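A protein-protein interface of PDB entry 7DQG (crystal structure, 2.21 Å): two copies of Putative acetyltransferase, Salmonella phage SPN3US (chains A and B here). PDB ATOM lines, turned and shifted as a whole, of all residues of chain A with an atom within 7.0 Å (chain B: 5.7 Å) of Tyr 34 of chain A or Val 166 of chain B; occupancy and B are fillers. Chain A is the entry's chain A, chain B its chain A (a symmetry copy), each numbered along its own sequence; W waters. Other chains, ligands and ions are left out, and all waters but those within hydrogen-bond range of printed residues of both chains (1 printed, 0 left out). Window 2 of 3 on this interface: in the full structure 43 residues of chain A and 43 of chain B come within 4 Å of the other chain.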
ATOM      1  N   VAL A  24     -27.588 -24.650   3.370  1.00  0.00           N
ATOM      2  CA  VAL A  24     -28.146 -24.526   4.710  1.00  0.00           C
ATOM      3  C   VAL A  24     -29.535 -25.150   4.716  1.00  0.00           C
ATOM      4  O   VAL A  24     -30.412 -24.740   3.947  1.00  0.00           O
ATOM      5  CB  VAL A  24     -28.200 -23.058   5.157  1.00  0.00           C
ATOM      6  CG1 VAL A  24     -28.921 -22.938   6.489  1.00  0.00           C
ATOM      7  CG2 VAL A  24     -26.795 -22.482   5.254  1.00  0.00           C
ATOM      8  N   ILE A  29     -32.244 -24.261  10.956  1.00  0.00           N
ATOM      9  CA  ILE A  29     -31.584 -23.051  11.440  1.00  0.00           C
ATOM     10  C   ILE A  29     -32.083 -22.777  12.854  1.00  0.00           C
ATOM     11  O   ILE A  29     -33.298 -22.638  13.063  1.00  0.00           O
ATOM     12  CB  ILE A  29     -31.848 -21.852  10.516  1.00  0.00           C
ATOM     13  CG1 ILE A  29     -31.346 -22.140   9.101  1.00  0.00           C
ATOM     14  CG2 ILE A  29     -31.190 -20.596  11.069  1.00  0.00           C
ATOM     15  CD1 ILE A  29     -31.531 -20.977   8.148  1.00  0.00           C
ATOM     16  N   PRO A  30     -31.196 -22.700  13.851  1.00  0.00           N
ATOM     17  CA  PRO A  30     -31.653 -22.478  15.231  1.00  0.00           C
ATOM     18  C   PRO A  30     -32.347 -21.136  15.404  1.00  0.00           C
ATOM     19  O   PRO A  30     -31.701 -20.083  15.377  1.00  0.00           O
ATOM     20  CB  PRO A  30     -30.356 -22.556  16.049  1.00  0.00           C
ATOM     21  CG  PRO A  30     -29.265 -22.265  15.069  1.00  0.00           C
ATOM     22  CD  PRO A  30     -29.732 -22.824  13.759  1.00  0.00           C
ATOM     23  N   ALA A  31     -33.672 -21.171  15.584  1.00  0.00           N
ATOM     24  CA  ALA A  31     -34.449 -19.939  15.664  1.00  0.00           C
ATOM     25  C   ALA A  31     -34.114 -19.132  16.911  1.00  0.00           C
ATOM     26  O   ALA A  31     -34.278 -17.907  16.915  1.00  0.00           O
ATOM     27  CB  ALA A  31     -35.943 -20.257  15.626  1.00  0.00           C
ATOM     28  N   ASN A  32     -33.649 -19.792  17.974  1.00  0.00           N
ATOM     29  CA  ASN A  32     -33.291 -19.066  19.187  1.00  0.00           C
ATOM     30  C   ASN A  32     -32.048 -18.208  18.986  1.00  0.00           C
ATOM     31  O   ASN A  32     -31.878 -17.196  19.678  1.00  0.00           O
ATOM     32  CB  ASN A  32     -33.080 -20.047  20.341  1.00  0.00           C
ATOM     33  CG  ASN A  32     -32.141 -21.183  19.979  1.00  0.00           C
ATOM     34  OD1 ASN A  32     -32.175 -21.703  18.863  1.00  0.00           O
ATOM     35  ND2 ASN A  32     -31.295 -21.575  20.925  1.00  0.00           N
ATOM     36  N   VAL A  33     -31.183 -18.581  18.048  1.00  0.00           N
ATOM     37  CA  VAL A  33     -29.941 -17.861  17.802  1.00  0.00           C
ATOM     38  C   VAL A  33     -30.081 -16.865  16.657  1.00  0.00           C
ATOM     39  O   VAL A  33     -29.566 -15.749  16.739  1.00  0.00           O
ATOM     40  CB  VAL A  33     -28.791 -18.858  17.535  1.00  0.00           C
ATOM     41  CG1 VAL A  33     -27.491 -18.116  17.268  1.00  0.00           C
ATOM     42  CG2 VAL A  33     -28.630 -19.812  18.707  1.00  0.00           C
ATOM     43  N   TYR A  34     -30.779 -17.239  15.583  1.00  0.00           N
ATOM     44  CA  TYR A  34     -30.917 -16.402  14.393  1.00  0.00           C
ATOM     45  C   TYR A  34     -32.393 -16.155  14.093  1.00  0.00           C
ATOM     46  O   TYR A  34     -32.918 -16.635  13.078  1.00  0.00           O
ATOM     47  CB  TYR A  34     -30.224 -17.045  13.194  1.00  0.00           C
ATOM     48  CG  TYR A  34     -28.790 -17.436  13.466  1.00  0.00           C
ATOM     49  CD1 TYR A  34     -27.807 -16.469  13.624  1.00  0.00           C
ATOM     50  CD2 TYR A  34     -28.422 -18.770  13.576  1.00  0.00           C
ATOM     51  CE1 TYR A  34     -26.496 -16.817  13.876  1.00  0.00           C
ATOM     52  CE2 TYR A  34     -27.114 -19.130  13.830  1.00  0.00           C
ATOM     53  CZ  TYR A  34     -26.155 -18.149  13.978  1.00  0.00           C
ATOM     54  OH  TYR A  34     -24.848 -18.500  14.233  1.00  0.00           O
ATOM     55  N   PRO A  35     -33.088 -15.381  14.941  1.00  0.00           N
ATOM     56  CA  PRO A  35     -34.528 -15.170  14.733  1.00  0.00           C
ATOM     57  C   PRO A  35     -34.838 -14.399  13.461  1.00  0.00           C
ATOM     58  O   PRO A  35     -35.719 -14.793  12.690  1.00  0.00           O
ATOM     59  CB  PRO A  35     -34.956 -14.381  15.981  1.00  0.00           C
ATOM     60  CG  PRO A  35     -33.799 -14.462  16.936  1.00  0.00           C
ATOM     61  CD  PRO A  35     -32.582 -14.610  16.087  1.00  0.00           C
ATOM     62  N   GLU A  36     -34.118 -13.297  13.229  1.00  0.00           N
ATOM     63  CA  GLU A  36     -34.397 -12.463  12.063  1.00  0.00           C
ATOM     64  C   GLU A  36     -34.085 -13.196  10.762  1.00  0.00           C
ATOM     65  O   GLU A  36     -34.843 -13.092   9.790  1.00  0.00           O
ATOM     66  CB  GLU A  36     -33.605 -11.161  12.144  1.00  0.00           C
ATOM     67  CG  GLU A  36     -33.751 -10.425  13.464  1.00  0.00           C
ATOM     68  CD  GLU A  36     -32.458 -10.388  14.253  1.00  0.00           C
ATOM     69  OE1 GLU A  36     -31.949 -11.472  14.618  1.00  0.00           O
ATOM     70  OE2 GLU A  36     -31.950  -9.275  14.503  1.00  0.00           O
ATOM     71  N   LEU A  37     -32.974 -13.937  10.720  1.00  0.00           N
ATOM     72  CA  LEU A  37     -32.643 -14.692   9.516  1.00  0.00           C
ATOM     73  C   LEU A  37     -33.705 -15.743   9.218  1.00  0.00           C
ATOM     74  O   LEU A  37     -34.069 -15.956   8.055  1.00  0.00           O
ATOM     75  CB  LEU A  37     -31.268 -15.346   9.660  1.00  0.00           C
ATOM     76  CG  LEU A  37     -30.882 -16.292   8.519  1.00  0.00           C
ATOM     77  CD1 LEU A  37     -30.708 -15.520   7.223  1.00  0.00           C
ATOM     78  CD2 LEU A  37     -29.626 -17.081   8.854  1.00  0.00           C
ATOM     79  N   VAL A  38     -34.211 -16.413  10.258  1.00  0.00           N
ATOM     80  CA  VAL A  38     -35.271 -17.399  10.065  1.00  0.00           C
ATOM     81  C   VAL A  38     -36.520 -16.731   9.503  1.00  0.00           C
ATOM     82  O   VAL A  38     -37.182 -17.269   8.606  1.00  0.00           O
ATOM     83  CB  VAL A  38     -35.564 -18.134  11.388  1.00  0.00           C
ATOM     84  CG1 VAL A  38     -36.886 -18.886  11.311  1.00  0.00           C
ATOM     85  CG2 VAL A  38     -34.433 -19.089  11.724  1.00  0.00           C
ATOM     86  N   GLU A  39     -36.850 -15.539  10.007  1.00  0.00           N
ATOM     87  CA  GLU A  39     -38.014 -14.819   9.503  1.00  0.00           C
ATOM     88  C   GLU A  39     -37.805 -14.366   8.062  1.00  0.00           C
ATOM     89  O   GLU A  39     -38.710 -14.492   7.228  1.00  0.00           O
ATOM     90  CB  GLU A  39     -38.320 -13.624  10.407  1.00  0.00           C
ATOM     91  CG  GLU A  39     -39.351 -12.657   9.839  1.00  0.00           C
ATOM     92  CD  GLU A  39     -40.693 -13.317   9.569  1.00  0.00           C
ATOM     93  OE1 GLU A  39     -41.078 -14.227  10.334  1.00  0.00           O
ATOM     94  OE2 GLU A  39     -41.362 -12.925   8.590  1.00  0.00           O
ATOM     95  N   MET A  56     -23.403 -21.510   1.442  1.00  0.00           N
ATOM     96  CA  MET A  56     -22.181 -20.930   1.977  1.00  0.00           C
ATOM     97  C   MET A  56     -20.975 -21.503   1.243  1.00  0.00           C
ATOM     98  O   MET A  56     -20.979 -22.661   0.816  1.00  0.00           O
ATOM     99  CB  MET A  56     -22.052 -21.190   3.481  1.00  0.00           C
ATOM    100  CG  MET A  56     -23.032 -20.400   4.336  1.00  0.00           C
ATOM    101  SD  MET A  56     -22.701 -20.546   6.106  1.00  0.00           S
ATOM    102  CE  MET A  56     -22.788 -22.322   6.320  1.00  0.00           C
ATOM    103  N   VAL A  63     -16.036 -18.663   6.281  1.00  0.00           N
ATOM    104  CA  VAL A  63     -17.095 -18.591   5.278  1.00  0.00           C
ATOM    105  C   VAL A  63     -16.744 -17.421   4.362  1.00  0.00           C
ATOM    106  O   VAL A  63     -16.928 -16.257   4.721  1.00  0.00           O
ATOM    107  CB  VAL A  63     -18.480 -18.430   5.909  1.00  0.00           C
ATOM    108  CG1 VAL A  63     -19.544 -18.332   4.822  1.00  0.00           C
ATOM    109  CG2 VAL A  63     -18.771 -19.599   6.838  1.00  0.00           C
ATOM    110  N   HIS B 161     -23.648 -11.820   9.950  1.00  0.00           N
ATOM    111  CA  HIS B 161     -23.534 -12.348  11.307  1.00  0.00           C
ATOM    112  C   HIS B 161     -23.659 -13.865  11.323  1.00  0.00           C
ATOM    113  O   HIS B 161     -22.941 -14.547  12.063  1.00  0.00           O
ATOM    114  CB  HIS B 161     -24.592 -11.712  12.211  1.00  0.00           C
ATOM    115  CG  HIS B 161     -24.660 -12.321  13.579  1.00  0.00           C
ATOM    116  ND1 HIS B 161     -25.746 -13.051  14.016  1.00  0.00           N
ATOM    117  CD2 HIS B 161     -23.777 -12.310  14.606  1.00  0.00           C
ATOM    118  CE1 HIS B 161     -25.528 -13.462  15.254  1.00  0.00           C
ATOM    119  NE2 HIS B 161     -24.341 -13.027  15.634  1.00  0.00           N
ATOM    120  N   TYR B 162     -24.564 -14.416  10.510  1.00  0.00           N
ATOM    121  CA  TYR B 162     -24.717 -15.865  10.454  1.00  0.00           C
ATOM    122  C   TYR B 162     -23.465 -16.529   9.894  1.00  0.00           C
ATOM    123  O   TYR B 162     -22.989 -17.528  10.445  1.00  0.00           O
ATOM    124  CB  TYR B 162     -25.944 -16.232   9.617  1.00  0.00           C
ATOM    125  CG  TYR B 162     -26.124 -17.720   9.399  1.00  0.00           C
ATOM    126  CD1 TYR B 162     -26.761 -18.510  10.349  1.00  0.00           C
ATOM    127  CD2 TYR B 162     -25.659 -18.336   8.241  1.00  0.00           C
ATOM    128  CE1 TYR B 162     -26.930 -19.872  10.153  1.00  0.00           C
ATOM    129  CE2 TYR B 162     -25.822 -19.696   8.037  1.00  0.00           C
ATOM    130  CZ  TYR B 162     -26.458 -20.459   8.997  1.00  0.00           C
ATOM    131  OH  TYR B 162     -26.621 -21.810   8.797  1.00  0.00           O
ATOM    132  N   ALA B 163     -22.915 -15.979   8.807  1.00  0.00           N
ATOM    133  CA  ALA B 163     -21.747 -16.583   8.172  1.00  0.00           C
ATOM    134  C   ALA B 163     -20.555 -16.627   9.121  1.00  0.00           C
ATOM    135  O   ALA B 163     -19.794 -17.601   9.131  1.00  0.00           O
ATOM    136  CB  ALA B 163     -21.390 -15.815   6.898  1.00  0.00           C
ATOM    137  N   GLU B 164     -20.380 -15.584   9.933  1.00  0.00           N
ATOM    138  CA  GLU B 164     -19.240 -15.529  10.840  1.00  0.00           C
ATOM    139  C   GLU B 164     -19.442 -16.394  12.080  1.00  0.00           C
ATOM    140  O   GLU B 164     -18.467 -16.929  12.618  1.00  0.00           O
ATOM    141  CB  GLU B 164     -18.973 -14.074  11.245  1.00  0.00           C
ATOM    142  CG  GLU B 164     -17.941 -13.888  12.353  1.00  0.00           C
ATOM    143  CD  GLU B 164     -16.524 -14.198  11.897  1.00  0.00           C
ATOM    144  OE1 GLU B 164     -16.208 -13.946  10.715  1.00  0.00           O
ATOM    145  OE2 GLU B 164     -15.726 -14.694  12.720  1.00  0.00           O
ATOM    146  N   SER B 165     -20.687 -16.569  12.530  1.00  0.00           N
ATOM    147  CA  SER B 165     -20.948 -17.120  13.856  1.00  0.00           C
ATOM    148  C   SER B 165     -21.413 -18.571  13.858  1.00  0.00           C
ATOM    149  O   SER B 165     -21.295 -19.231  14.899  1.00  0.00           O
ATOM    150  CB  SER B 165     -21.998 -16.270  14.584  1.00  0.00           C
ATOM    151  OG  SER B 165     -23.210 -16.216  13.853  1.00  0.00           O
ATOM    152  N   VAL B 166     -21.937 -19.085  12.751  1.00  0.00           N
ATOM    153  CA  VAL B 166     -22.578 -20.407  12.797  1.00  0.00           C
ATOM    154  C   VAL B 166     -21.512 -21.488  12.962  1.00  0.00           C
ATOM    155  O   VAL B 166     -20.466 -21.439  12.287  1.00  0.00           O
ATOM    156  CB  VAL B 166     -23.430 -20.639  11.541  1.00  0.00           C
ATOM    157  CG1 VAL B 166     -22.574 -20.706  10.278  1.00  0.00           C
ATOM    158  CG2 VAL B 166     -24.270 -21.903  11.692  1.00  0.00           C
ATOM    159  N   PRO B 167     -21.705 -22.451  13.862  1.00  0.00           N
ATOM    160  CA  PRO B 167     -20.746 -23.558  13.967  1.00  0.00           C
ATOM    161  C   PRO B 167     -20.825 -24.474  12.755  1.00  0.00           C
ATOM    162  O   PRO B 167     -21.911 -24.783  12.256  1.00  0.00           O
ATOM    163  CB  PRO B 167     -21.176 -24.285  15.248  1.00  0.00           C
ATOM    164  CG  PRO B 167     -21.996 -23.280  16.007  1.00  0.00           C
ATOM    165  CD  PRO B 167     -22.682 -22.459  14.963  1.00  0.00           C
ATOM    166  N   ILE B 168     -19.658 -24.902  12.280  1.00  0.00           N
ATOM    167  CA  ILE B 168     -19.543 -25.778  11.120  1.00  0.00           C
ATOM    168  C   ILE B 168     -18.558 -26.887  11.461  1.00  0.00           C
ATOM    169  O   ILE B 168     -17.367 -26.620  11.667  1.00  0.00           O
ATOM    170  CB  ILE B 168     -19.081 -25.019   9.861  1.00  0.00           C
ATOM    171  CG1 ILE B 168     -19.961 -23.793   9.613  1.00  0.00           C
ATOM    172  CG2 ILE B 168     -19.097 -25.943   8.651  1.00  0.00           C
ATOM    173  CD1 ILE B 168     -19.457 -22.898   8.503  1.00  0.00           C
HETATM  174  O   HOH W   1     -16.502 -17.201   8.693  1.00  0.00           O
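OH of Tyr 34 of chain A sits at hydrogen-bond distance from OG of Ser 165 of chain B, at 2.8 Å. OH of Tyr 34 of chain A lies close to N of Val 166 of chain B, 3.3 Å away.
OG of Ser 165 of chain B lies within hydrogen-bond range of O of His 161 of chain B (2.5 Å).
Among the printed residues, pairs that only touch across the chains: Val 24 of chain A with Tyr 162 of chain B, Tyr 34 of chain A with His 161 of chain B, Tyr 34 of chain A with Tyr 162 of chain B, Leu 37 of chain A with Tyr 162 of chain B, Met 56 of chain A with Tyr 162 of chain B, Val 63 of chain A with Ala 163 of chain B and Val 63 of chain A with Ile 168 of chain B.
Ile 29 of chain A touches none of the printed residues of chain B. Tyr 34 of chain A touches just these residues of chain B: His 161 (3.8 Å), Tyr 162 (3.6 Å), Ser 165 (2.8 Å) and Val 166 (3.3 Å). Of the printed residues of chain B, Leu 37 of chain A touches Tyr 162. Of the printed residues of chain B, Val 63 of chain A touches Ala 163 and Ile 168. Printed residues of chain A within 4 Å of Ser 165 of chain B: Tyr 34. Of the printed residues of chain A, Val 166 of chain B touches Tyr 34. Pro 167 of chain B touches none of the printed residues of chain A. The nearest residue of chain A that does not touch Val 166 of chain B is Met 56 of chain A (4.2 Å). The nearest printed residue of chain A that does not touch His 161 of chain B is Val 33 of chain A (4.9 Å).
Of the 14 printed residues of chain A, 5 touch a printed residue of chain B. Hydrophobic or aromatic side chains of chain A within 4 Å of the printed part of chain B: Val 24, Tyr 34, Leu 37, Met 56 and Val 63. Among the printed residues, no Asp or Glu carboxylate lies within 4 Å of a Lys or Arg side-chain nitrogen of the other chain.
No position is printed for both chains. Of the 9 pairs that touch across the chains among the printed residues, none has its exchanged pair printed and touching as well.
Water W1 bridges N of Val 63 of chain A and O of Ala 163 of chain B.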
